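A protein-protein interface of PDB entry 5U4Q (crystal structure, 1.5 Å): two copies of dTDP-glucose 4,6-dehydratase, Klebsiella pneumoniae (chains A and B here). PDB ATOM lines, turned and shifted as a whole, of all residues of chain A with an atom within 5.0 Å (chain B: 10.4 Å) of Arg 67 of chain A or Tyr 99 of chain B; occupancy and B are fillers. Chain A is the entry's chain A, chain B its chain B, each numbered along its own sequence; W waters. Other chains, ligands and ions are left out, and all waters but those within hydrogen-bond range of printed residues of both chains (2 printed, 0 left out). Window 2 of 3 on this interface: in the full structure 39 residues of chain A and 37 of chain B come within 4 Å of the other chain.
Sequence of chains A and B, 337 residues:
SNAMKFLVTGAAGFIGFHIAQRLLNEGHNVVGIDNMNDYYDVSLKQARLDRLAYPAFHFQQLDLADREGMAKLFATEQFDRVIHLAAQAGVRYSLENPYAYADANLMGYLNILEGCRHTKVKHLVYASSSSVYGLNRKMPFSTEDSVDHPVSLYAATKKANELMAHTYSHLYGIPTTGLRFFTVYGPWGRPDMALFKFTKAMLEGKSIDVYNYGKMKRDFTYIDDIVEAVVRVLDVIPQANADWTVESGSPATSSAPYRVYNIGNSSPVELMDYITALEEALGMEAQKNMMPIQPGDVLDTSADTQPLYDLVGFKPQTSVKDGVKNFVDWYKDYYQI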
ATOM      1  N   ALA A  65      22.713 -13.058 -24.574  1.00  0.00           N
ATOM      2  CA  ALA A  65      21.752 -12.213 -25.262  1.00  0.00           C
ATOM      3  C   ALA A  65      20.345 -12.281 -24.689  1.00  0.00           C
ATOM      4  O   ALA A  65      19.472 -11.541 -25.144  1.00  0.00           O
ATOM      5  CB  ALA A  65      21.723 -12.590 -26.723  1.00  0.00           C
ATOM      6  N   ASP A  66      20.132 -13.141 -23.702  1.00  0.00           N
ATOM      7  CA  ASP A  66      18.820 -13.309 -23.035  1.00  0.00           C
ATOM      8  C   ASP A  66      18.738 -12.195 -21.984  1.00  0.00           C
ATOM      9  O   ASP A  66      19.225 -12.343 -20.863  1.00  0.00           O
ATOM     10  CB  ASP A  66      18.751 -14.717 -22.435  1.00  0.00           C
ATOM     11  CG  ASP A  66      17.446 -15.026 -21.705  1.00  0.00           C
ATOM     12  OD1 ASP A  66      16.620 -14.125 -21.456  1.00  0.00           O
ATOM     13  OD2 ASP A  66      17.267 -16.207 -21.372  1.00  0.00           O
ATOM     14  N   ARG A  67      18.111 -11.078 -22.351  1.00  0.00           N
ATOM     15  CA  ARG A  67      18.071  -9.901 -21.492  1.00  0.00           C
ATOM     16  C   ARG A  67      17.426 -10.178 -20.144  1.00  0.00           C
ATOM     17  O   ARG A  67      17.985  -9.829 -19.109  1.00  0.00           O
ATOM     18  CB  ARG A  67      17.344  -8.724 -22.168  1.00  0.00           C
ATOM     19  CG  ARG A  67      17.275  -7.496 -21.262  1.00  0.00           C
ATOM     20  CD  ARG A  67      16.575  -6.316 -21.896  1.00  0.00           C
ATOM     21  NE  ARG A  67      16.364  -5.265 -20.901  1.00  0.00           N
ATOM     22  CZ  ARG A  67      15.666  -4.148 -21.107  1.00  0.00           C
ATOM     23  NH1 ARG A  67      15.105  -3.908 -22.294  1.00  0.00           N
ATOM     24  NH2 ARG A  67      15.544  -3.259 -20.124  1.00  0.00           N
ATOM     25  N   GLU A  68      16.245 -10.801 -20.148  1.00  0.00           N
ATOM     26  CA  GLU A  68      15.557 -11.084 -18.888  1.00  0.00           C
ATOM     27  C   GLU A  68      16.327 -12.111 -18.066  1.00  0.00           C
ATOM     28  O   GLU A  68      16.441 -11.967 -16.840  1.00  0.00           O
ATOM     29  CB  GLU A  68      14.104 -11.546 -19.120  1.00  0.00           C
ATOM     30  CG  GLU A  68      13.364 -11.839 -17.821  1.00  0.00           C
ATOM     31  CD  GLU A  68      11.877 -12.061 -17.986  1.00  0.00           C
ATOM     32  OE1 GLU A  68      11.398 -12.221 -19.133  1.00  0.00           O
ATOM     33  OE2 GLU A  68      11.186 -12.065 -16.944  1.00  0.00           O
ATOM     34  N   GLY A  69      16.849 -13.141 -18.737  1.00  0.00           N
ATOM     35  CA  GLY A  69      17.634 -14.198 -18.044  1.00  0.00           C
ATOM     36  C   GLY A  69      18.894 -13.619 -17.394  1.00  0.00           C
ATOM     37  O   GLY A  69      19.265 -13.973 -16.279  1.00  0.00           O
ATOM     38  N   MET A  70      19.567 -12.736 -18.119  1.00  0.00           N
ATOM     39  CA  MET A  70      20.752 -12.078 -17.570  1.00  0.00           C
ATOM     40  C   MET A  70      20.426 -11.178 -16.403  1.00  0.00           C
ATOM     41  O   MET A  70      21.104 -11.184 -15.372  1.00  0.00           O
ATOM     42  CB  MET A  70      21.452 -11.297 -18.672  1.00  0.00           C
ATOM     43  CG  MET A  70      22.143 -12.227 -19.655  1.00  0.00           C
ATOM     44  SD  MET A  70      23.778 -13.061 -18.959  1.00  0.00           S
ATOM     45  CE  MET A  70      24.876 -11.451 -19.099  1.00  0.00           C
ATOM     46  N   ALA A  71      19.351 -10.407 -16.530  1.00  0.00           N
ATOM     47  CA  ALA A  71      18.923  -9.546 -15.431  1.00  0.00           C
ATOM     48  C   ALA A  71      18.589 -10.366 -14.175  1.00  0.00           C
ATOM     49  O   ALA A  71      18.990  -9.990 -13.069  1.00  0.00           O
ATOM     50  CB  ALA A  71      17.724  -8.707 -15.860  1.00  0.00           C
ATOM     51  N   MET A 107      25.407  -7.149 -27.959  1.00  0.00           N
ATOM     52  CA  MET A 107      24.247  -7.150 -27.039  1.00  0.00           C
ATOM     53  C   MET A 107      24.570  -7.866 -25.760  1.00  0.00           C
ATOM     54  O   MET A 107      24.198  -7.416 -24.660  1.00  0.00           O
ATOM     55  CB  MET A 107      23.080  -7.852 -27.713  1.00  0.00           C
ATOM     56  CG  MET A 107      21.810  -7.964 -26.867  1.00  0.00           C
ATOM     57  SD  MET A 107      21.015  -6.213 -26.453  1.00  0.00           S
ATOM     58  CE  MET A 107      20.492  -5.711 -28.287  1.00  0.00           C
ATOM     59  N   LEU A 110      26.489  -5.660 -23.464  1.00  0.00           N
ATOM     60  CA  LEU A 110      25.636  -4.664 -22.822  1.00  0.00           C
ATOM     61  C   LEU A 110      24.881  -5.281 -21.648  1.00  0.00           C
ATOM     62  O   LEU A 110      24.778  -4.638 -20.612  1.00  0.00           O
ATOM     63  CB  LEU A 110      24.653  -4.035 -23.801  1.00  0.00           C
ATOM     64  CG  LEU A 110      23.758  -2.933 -23.199  1.00  0.00           C
ATOM     65  CD1 LEU A 110      24.536  -1.798 -22.553  1.00  0.00           C
ATOM     66  CD2 LEU A 110      22.789  -2.405 -24.252  1.00  0.00           C
ATOM     67  N   ASN A 111      24.372  -6.513 -21.801  1.00  0.00           N
ATOM     68  CA  ASN A 111      23.668  -7.173 -20.673  1.00  0.00           C
ATOM     69  C   ASN A 111      24.599  -7.314 -19.475  1.00  0.00           C
ATOM     70  O   ASN A 111      24.183  -7.119 -18.335  1.00  0.00           O
ATOM     71  CB  ASN A 111      23.050  -8.509 -21.100  1.00  0.00           C
ATOM     72  CG  ASN A 111      21.925  -8.316 -22.092  1.00  0.00           C
ATOM     73  OD1 ASN A 111      21.338  -7.229 -22.145  1.00  0.00           O
ATOM     74  ND2 ASN A 111      21.634  -9.330 -22.906  1.00  0.00           N
ATOM     75  N   GLU A 114      25.002  -3.746 -17.948  1.00  0.00           N
ATOM     76  CA  GLU A 114      23.760  -3.382 -17.238  1.00  0.00           C
ATOM     77  C   GLU A 114      23.656  -4.106 -15.918  1.00  0.00           C
ATOM     78  O   GLU A 114      23.281  -3.499 -14.900  1.00  0.00           O
ATOM     79  CB  GLU A 114      22.542  -3.612 -18.120  1.00  0.00           C
ATOM     80  CG  GLU A 114      22.328  -2.477 -19.108  1.00  0.00           C
ATOM     81  CD  GLU A 114      21.876  -1.194 -18.420  1.00  0.00           C
ATOM     82  OE1 GLU A 114      20.716  -1.209 -17.954  1.00  0.00           O
ATOM     83  OE2 GLU A 114      22.626  -0.199 -18.367  1.00  0.00           O
ATOM     84  N   ASN B  35      11.057   2.928 -38.677  1.00  0.00           N
ATOM     85  CA  ASN B  35      10.143   2.131 -37.835  1.00  0.00           C
ATOM     86  C   ASN B  35       9.064   2.957 -37.136  1.00  0.00           C
ATOM     87  O   ASN B  35       8.243   2.391 -36.394  1.00  0.00           O
ATOM     88  CB  ASN B  35      10.906   1.244 -36.851  1.00  0.00           C
ATOM     89  CG  ASN B  35      11.546   2.006 -35.723  1.00  0.00           C
ATOM     90  OD1 ASN B  35      11.495   3.230 -35.670  1.00  0.00           O
ATOM     91  ND2 ASN B  35      12.098   1.263 -34.764  1.00  0.00           N
ATOM     92  N   ASP B  63      12.152  -2.247 -39.395  1.00  0.00           N
ATOM     93  CA  ASP B  63      13.054  -1.997 -38.304  1.00  0.00           C
ATOM     94  C   ASP B  63      14.448  -2.441 -38.736  1.00  0.00           C
ATOM     95  O   ASP B  63      14.632  -3.523 -39.285  1.00  0.00           O
ATOM     96  CB  ASP B  63      12.641  -2.769 -37.069  1.00  0.00           C
ATOM     97  CG  ASP B  63      13.255  -2.213 -35.829  1.00  0.00           C
ATOM     98  OD1 ASP B  63      14.491  -2.269 -35.697  1.00  0.00           O
ATOM     99  OD2 ASP B  63      12.501  -1.691 -34.980  1.00  0.00           O
ATOM    100  N   ALA B  65      16.692  -3.624 -36.973  1.00  0.00           N
ATOM    101  CA  ALA B  65      17.072  -4.841 -36.240  1.00  0.00           C
ATOM    102  C   ALA B  65      16.404  -6.103 -36.801  1.00  0.00           C
ATOM    103  O   ALA B  65      16.705  -7.198 -36.351  1.00  0.00           O
ATOM    104  CB  ALA B  65      16.751  -4.679 -34.775  1.00  0.00           C
ATOM    105  N   ALA B  87      18.720   5.804 -36.332  1.00  0.00           N
ATOM    106  CA  ALA B  87      19.456   5.526 -35.095  1.00  0.00           C
ATOM    107  C   ALA B  87      18.618   6.056 -33.955  1.00  0.00           C
ATOM    108  O   ALA B  87      17.694   6.860 -34.157  1.00  0.00           O
ATOM    109  CB  ALA B  87      20.809   6.245 -35.080  1.00  0.00           C
ATOM    110  N   GLN B  88      18.946   5.608 -32.748  1.00  0.00           N
ATOM    111  CA  GLN B  88      18.379   6.146 -31.545  1.00  0.00           C
ATOM    112  C   GLN B  88      19.346   7.253 -31.162  1.00  0.00           C
ATOM    113  O   GLN B  88      20.510   6.992 -30.844  1.00  0.00           O
ATOM    114  CB  GLN B  88      18.304   5.096 -30.435  1.00  0.00           C
ATOM    115  CG  GLN B  88      17.692   5.649 -29.155  1.00  0.00           C
ATOM    116  CD  GLN B  88      16.371   6.320 -29.453  1.00  0.00           C
ATOM    117  OE1 GLN B  88      15.478   5.698 -30.028  1.00  0.00           O
ATOM    118  NE2 GLN B  88      16.256   7.611 -29.116  1.00  0.00           N
ATOM    119  N   LEU B  95      21.636   7.178 -20.886  1.00  0.00           N
ATOM    120  CA  LEU B  95      21.578   6.586 -19.544  1.00  0.00           C
ATOM    121  C   LEU B  95      20.278   5.811 -19.343  1.00  0.00           C
ATOM    122  O   LEU B  95      20.263   4.727 -18.725  1.00  0.00           O
ATOM    123  CB  LEU B  95      21.758   7.663 -18.459  1.00  0.00           C
ATOM    124  CG  LEU B  95      23.191   8.197 -18.280  1.00  0.00           C
ATOM    125  CD1 LEU B  95      23.730   8.833 -19.562  1.00  0.00           C
ATOM    126  CD2 LEU B  95      23.279   9.180 -17.119  1.00  0.00           C
ATOM    127  N   GLU B  96      19.190   6.382 -19.856  1.00  0.00           N
ATOM    128  CA  GLU B  96      17.884   5.749 -19.802  1.00  0.00           C
ATOM    129  C   GLU B  96      17.600   5.136 -21.162  1.00  0.00           C
ATOM    130  O   GLU B  96      17.739   5.785 -22.200  1.00  0.00           O
ATOM    131  CB  GLU B  96      16.796   6.746 -19.405  1.00  0.00           C
ATOM    132  CG  GLU B  96      16.966   7.257 -17.981  1.00  0.00           C
ATOM    133  CD  GLU B  96      15.882   8.224 -17.549  1.00  0.00           C
ATOM    134  OE1 GLU B  96      15.006   8.569 -18.374  1.00  0.00           O
ATOM    135  OE2 GLU B  96      15.913   8.643 -16.371  1.00  0.00           O
ATOM    136  N   ASN B  97      17.224   3.867 -21.120  1.00  0.00           N
ATOM    137  CA  ASN B  97      16.903   3.059 -22.289  1.00  0.00           C
ATOM    138  C   ASN B  97      18.143   2.656 -23.123  1.00  0.00           C
ATOM    139  O   ASN B  97      18.192   2.880 -24.328  1.00  0.00           O
ATOM    140  CB  ASN B  97      15.826   3.731 -23.150  1.00  0.00           C
ATOM    141  CG  ASN B  97      15.096   2.748 -24.045  1.00  0.00           C
ATOM    142  OD1 ASN B  97      15.486   1.585 -24.174  1.00  0.00           O
ATOM    143  ND2 ASN B  97      14.017   3.213 -24.667  1.00  0.00           N
ATOM    144  N   PRO B  98      19.130   2.002 -22.478  1.00  0.00           N
ATOM    145  CA  PRO B  98      20.301   1.570 -23.229  1.00  0.00           C
ATOM    146  C   PRO B  98      19.992   0.550 -24.342  1.00  0.00           C
ATOM    147  O   PRO B  98      20.684   0.519 -25.360  1.00  0.00           O
ATOM    148  CB  PRO B  98      21.201   0.926 -22.155  1.00  0.00           C
ATOM    149  CG  PRO B  98      20.600   1.264 -20.845  1.00  0.00           C
ATOM    150  CD  PRO B  98      19.165   1.553 -21.078  1.00  0.00           C
ATOM    151  N   TYR B  99      18.990  -0.296 -24.133  1.00  0.00           N
ATOM    152  CA  TYR B  99      18.649  -1.347 -25.093  1.00  0.00           C
ATOM    153  C   TYR B  99      18.230  -0.830 -26.462  1.00  0.00           C
ATOM    154  O   TYR B  99      18.500  -1.487 -27.461  1.00  0.00           O
ATOM    155  CB  TYR B  99      17.655  -2.340 -24.504  1.00  0.00           C
ATOM    156  CG  TYR B  99      18.335  -3.083 -23.397  1.00  0.00           C
ATOM    157  CD1 TYR B  99      19.189  -4.129 -23.695  1.00  0.00           C
ATOM    158  CD2 TYR B  99      18.213  -2.685 -22.072  1.00  0.00           C
ATOM    159  CE1 TYR B  99      19.869  -4.801 -22.701  1.00  0.00           C
ATOM    160  CE2 TYR B  99      18.905  -3.348 -21.061  1.00  0.00           C
ATOM    161  CZ  TYR B  99      19.727  -4.404 -21.387  1.00  0.00           C
ATOM    162  OH  TYR B  99      20.401  -5.063 -20.388  1.00  0.00           O
ATOM    163  N   ALA B 100      17.655   0.375 -26.484  1.00  0.00           N
ATOM    164  CA  ALA B 100      17.275   1.066 -27.735  1.00  0.00           C
ATOM    165  C   ALA B 100      18.490   1.400 -28.566  1.00  0.00           C
ATOM    166  O   ALA B 100      18.468   1.245 -29.778  1.00  0.00           O
ATOM    167  CB  ALA B 100      16.486   2.336 -27.435  1.00  0.00           C
ATOM    168  N   TYR B 101      19.571   1.790 -27.902  1.00  0.00           N
ATOM    169  CA  TYR B 101      20.803   2.125 -28.594  1.00  0.00           C
ATOM    170  C   TYR B 101      21.467   0.882 -29.143  1.00  0.00           C
ATOM    171  O   TYR B 101      21.979   0.887 -30.262  1.00  0.00           O
ATOM    172  CB  TYR B 101      21.750   2.892 -27.662  1.00  0.00           C
ATOM    173  CG  TYR B 101      21.199   4.246 -27.301  1.00  0.00           C
ATOM    174  CD1 TYR B 101      20.294   4.392 -26.262  1.00  0.00           C
ATOM    175  CD2 TYR B 101      21.519   5.367 -28.049  1.00  0.00           C
ATOM    176  CE1 TYR B 101      19.754   5.633 -25.940  1.00  0.00           C
ATOM    177  CE2 TYR B 101      20.988   6.609 -27.740  1.00  0.00           C
ATOM    178  CZ  TYR B 101      20.106   6.737 -26.685  1.00  0.00           C
ATOM    179  OH  TYR B 101      19.568   7.969 -26.392  1.00  0.00           O
ATOM    180  N   ALA B 102      21.470  -0.185 -28.373  1.00  0.00           N
ATOM    181  CA  ALA B 102      22.043  -1.419 -28.855  1.00  0.00           C
ATOM    182  C   ALA B 102      21.261  -1.924 -30.053  1.00  0.00           C
ATOM    183  O   ALA B 102      21.844  -2.310 -31.058  1.00  0.00           O
ATOM    184  CB  ALA B 102      22.040  -2.471 -27.753  1.00  0.00           C
ATOM    185  N   ASP B 103      19.946  -1.933 -29.933  1.00  0.00           N
ATOM    186  CA  ASP B 103      19.109  -2.457 -30.996  1.00  0.00           C
ATOM    187  C   ASP B 103      19.344  -1.682 -32.295  1.00  0.00           C
ATOM    188  O   ASP B 103      19.714  -2.265 -33.342  1.00  0.00           O
ATOM    189  CB  ASP B 103      17.602  -2.388 -30.640  1.00  0.00           C
ATOM    190  CG  ASP B 103      17.177  -3.395 -29.555  1.00  0.00           C
ATOM    191  OD1 ASP B 103      17.949  -4.313 -29.241  1.00  0.00           O
ATOM    192  OD2 ASP B 103      16.051  -3.263 -29.028  1.00  0.00           O
ATOM    193  N   ALA B 104      19.159  -0.386 -32.219  1.00  0.00           N
ATOM    194  CA  ALA B 104      19.220   0.449 -33.413  1.00  0.00           C
ATOM    195  C   ALA B 104      20.593   0.745 -33.897  1.00  0.00           C
ATOM    196  O   ALA B 104      20.860   0.720 -35.104  1.00  0.00           O
ATOM    197  CB  ALA B 104      18.491   1.754 -33.178  1.00  0.00           C
ATOM    198  N   ASN B 105      21.487   1.034 -32.967  1.00  0.00           N
ATOM    199  CA  ASN B 105      22.805   1.552 -33.355  1.00  0.00           C
ATOM    200  C   ASN B 105      23.881   0.495 -33.470  1.00  0.00           C
ATOM    201  O   ASN B 105      24.894   0.739 -34.117  1.00  0.00           O
ATOM    202  CB  ASN B 105      23.270   2.641 -32.376  1.00  0.00           C
ATOM    203  CG  ASN B 105      22.287   3.812 -32.234  1.00  0.00           C
ATOM    204  OD1 ASN B 105      21.200   3.803 -32.802  1.00  0.00           O
ATOM    205  ND2 ASN B 105      22.669   4.835 -31.442  1.00  0.00           N
ATOM    206  N   LEU B 106      23.706  -0.664 -32.838  1.00  0.00           N
ATOM    207  CA  LEU B 106      24.690  -1.727 -32.983  1.00  0.00           C
ATOM    208  C   LEU B 106      24.191  -2.825 -33.918  1.00  0.00           C
ATOM    209  O   LEU B 106      24.744  -3.020 -34.995  1.00  0.00           O
ATOM    210  CB  LEU B 106      25.105  -2.285 -31.615  1.00  0.00           C
ATOM    211  CG  LEU B 106      25.778  -1.317 -30.644  1.00  0.00           C
ATOM    212  CD1 LEU B 106      26.026  -1.949 -29.288  1.00  0.00           C
ATOM    213  CD2 LEU B 106      27.083  -0.817 -31.253  1.00  0.00           C
ATOM    214  N   MET B 107      23.131  -3.520 -33.514  1.00  0.00           N
ATOM    215  CA  MET B 107      22.589  -4.605 -34.334  1.00  0.00           C
ATOM    216  C   MET B 107      22.085  -4.067 -35.670  1.00  0.00           C
ATOM    217  O   MET B 107      22.331  -4.662 -36.717  1.00  0.00           O
ATOM    218  CB  MET B 107      21.426  -5.307 -33.618  1.00  0.00           C
ATOM    219  CG  MET B 107      21.552  -5.538 -32.101  1.00  0.00           C
ATOM    220  SD  MET B 107      23.115  -6.626 -31.594  1.00  0.00           S
ATOM    221  CE  MET B 107      22.396  -8.333 -32.267  1.00  0.00           C
ATOM    222  N   GLY B 108      21.378  -2.954 -35.631  1.00  0.00           N
ATOM    223  CA  GLY B 108      20.820  -2.325 -36.828  1.00  0.00           C
ATOM    224  C   GLY B 108      21.895  -1.937 -37.820  1.00  0.00           C
ATOM    225  O   GLY B 108      21.736  -2.114 -39.025  1.00  0.00           O
ATOM    226  N   LEU B 153      26.755   5.996 -23.793  1.00  0.00           N
ATOM    227  CA  LEU B 153      26.566   4.797 -24.585  1.00  0.00           C
ATOM    228  C   LEU B 153      26.278   5.174 -26.053  1.00  0.00           C
ATOM    229  O   LEU B 153      26.796   4.545 -26.965  1.00  0.00           O
ATOM    230  CB  LEU B 153      25.477   3.895 -23.988  1.00  0.00           C
ATOM    231  CG  LEU B 153      25.211   2.612 -24.782  1.00  0.00           C
ATOM    232  CD1 LEU B 153      26.455   1.751 -24.943  1.00  0.00           C
ATOM    233  CD2 LEU B 153      24.125   1.815 -24.090  1.00  0.00           C
ATOM    234  N   TYR B 154      25.506   6.237 -26.279  1.00  0.00           N
ATOM    235  CA  TYR B 154      25.240   6.728 -27.627  1.00  0.00           C
ATOM    236  C   TYR B 154      26.551   6.971 -28.376  1.00  0.00           C
ATOM    237  O   TYR B 154      26.754   6.485 -29.497  1.00  0.00           O
ATOM    238  CB  TYR B 154      24.415   8.007 -27.561  1.00  0.00           C
ATOM    239  CG  TYR B 154      24.303   8.737 -28.869  1.00  0.00           C
ATOM    240  CD1 TYR B 154      23.493   8.257 -29.879  1.00  0.00           C
ATOM    241  CD2 TYR B 154      24.999   9.903 -29.098  1.00  0.00           C
ATOM    242  CE1 TYR B 154      23.381   8.914 -31.089  1.00  0.00           C
ATOM    243  CE2 TYR B 154      24.900  10.579 -30.309  1.00  0.00           C
ATOM    244  CZ  TYR B 154      24.074  10.082 -31.301  1.00  0.00           C
ATOM    245  OH  TYR B 154      23.945  10.751 -32.518  1.00  0.00           O
ATOM    246  N   THR B 157      28.329   3.796 -29.296  1.00  0.00           N
ATOM    247  CA  THR B 157      27.719   3.105 -30.416  1.00  0.00           C
ATOM    248  C   THR B 157      28.111   3.755 -31.745  1.00  0.00           C
ATOM    249  O   THR B 157      28.310   3.053 -32.738  1.00  0.00           O
ATOM    250  CB  THR B 157      26.183   2.933 -30.301  1.00  0.00           C
ATOM    251  OG1 THR B 157      25.482   4.181 -30.425  1.00  0.00           O
ATOM    252  CG2 THR B 157      25.794   2.198 -29.017  1.00  0.00           C
HETATM  253  O   HOH W   1      18.151  -5.647 -18.385  1.00  0.00           O
HETATM  254  O   HOH W   2      19.952  -7.826 -19.063  1.00  0.00           O
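Water W2 lies within hydrogen-bond range of the backbone carbonyl oxygen (O) of Arg 67 of chain A, the side-chain hydroxyl (OH) of Tyr 99 of chain B and the side-chain amide oxygen (OD1) of Asn 111 of chain A.
Water W1 bridges OH of Tyr 99 of chain B and NE of Arg 67 of chain A.
Met 107 of chain B touches its own counterpart, Met 107 of chain A.
Positions printed for both chains: 65 and 107.
Of the 11 pairs that touch across the chains among the printed residues, 1 has its exchanged pair printed and touching as well.
Of the 22 printed residues of chain B, 6 touch a printed residue of chain A.
Hydrophobic or aromatic side chains of chain B that line the printed part of chain A: Pro 98, Tyr 99, Ala 102, Met 107 and Leu 153.
Of the 11 printed residues of chain A, 5 touch a printed residue of chain B.
Hydrophobic or aromatic side chains of chain A within 4 Å of the printed part of chain B: Met 107 and Leu 110.
Among the printed residues, 11 pairs touch across the chains.
The side-chain amide oxygen (OD1) of Asn 111 of chain A sits close to the side-chain hydroxyl (OH) of Tyr 99 of chain B (2.9 Å).
Among the printed residues, pairs that only touch across the chains: Met 107 of chain A with Asp 103 of chain B, Arg 67 of chain A with Tyr 99 of chain B, Glu 114 of chain A with Tyr 99 of chain B, Glu 114 of chain A with Pro 98 of chain B, Leu 110 of chain A with Ala 102 of chain B, Met 107 of chain A with Ala 102 of chain B, Leu 110 of chain A with Pro 98 of chain B, Met 107 of chain A with Tyr 99 of chain B, Leu 110 of chain A with Leu 153 of chain B and Met 107 of chain A with Met 107 of chain B.
The backbone NH (N) of Gly 108 of chain B sits at hydrogen-bond distance from the backbone carbonyl oxygen (O) of Asp 103 of chain B, 2.9 Å away.
The backbone NH (N) of Met 107 of chain B sits at hydrogen-bond distance from the backbone carbonyl oxygen (O) of Ala 102 of chain B (3.0 Å).
Arg 67 of chain A touches just one residue of chain B: Tyr 99 (3.1 Å).
Tyr 99 of chain B touches just these residues of chain A: Arg 67, Met 107, Asn 111 and Glu 114.
No residue of chain B comes within 4 Å of Asp 66 of chain A.
No residue of chain B comes within 4 Å of Ala 71 of chain A.
Of the printed residues of chain B, Leu 110 of chain A touches Pro 98 (3.8 Å), Ala 102 (3.6 Å) and Leu 153 (3.9 Å).
Of the printed residues of chain A, Pro 98 of chain B touches Leu 110 and Glu 114.
Printed residues of chain A within 4 Å of Asp 103 of chain B: Met 107.
Printed residues of chain B within 4 Å of Met 107 of chain A: Tyr 99 (3.9 Å), Ala 102 (3.6 Å), Asp 103 (3.1 Å) and Met 107 (3.96 Å).
The nearest residue of chain A that does not touch Tyr 99 of chain B is Leu 110 of chain A (4.03 Å).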
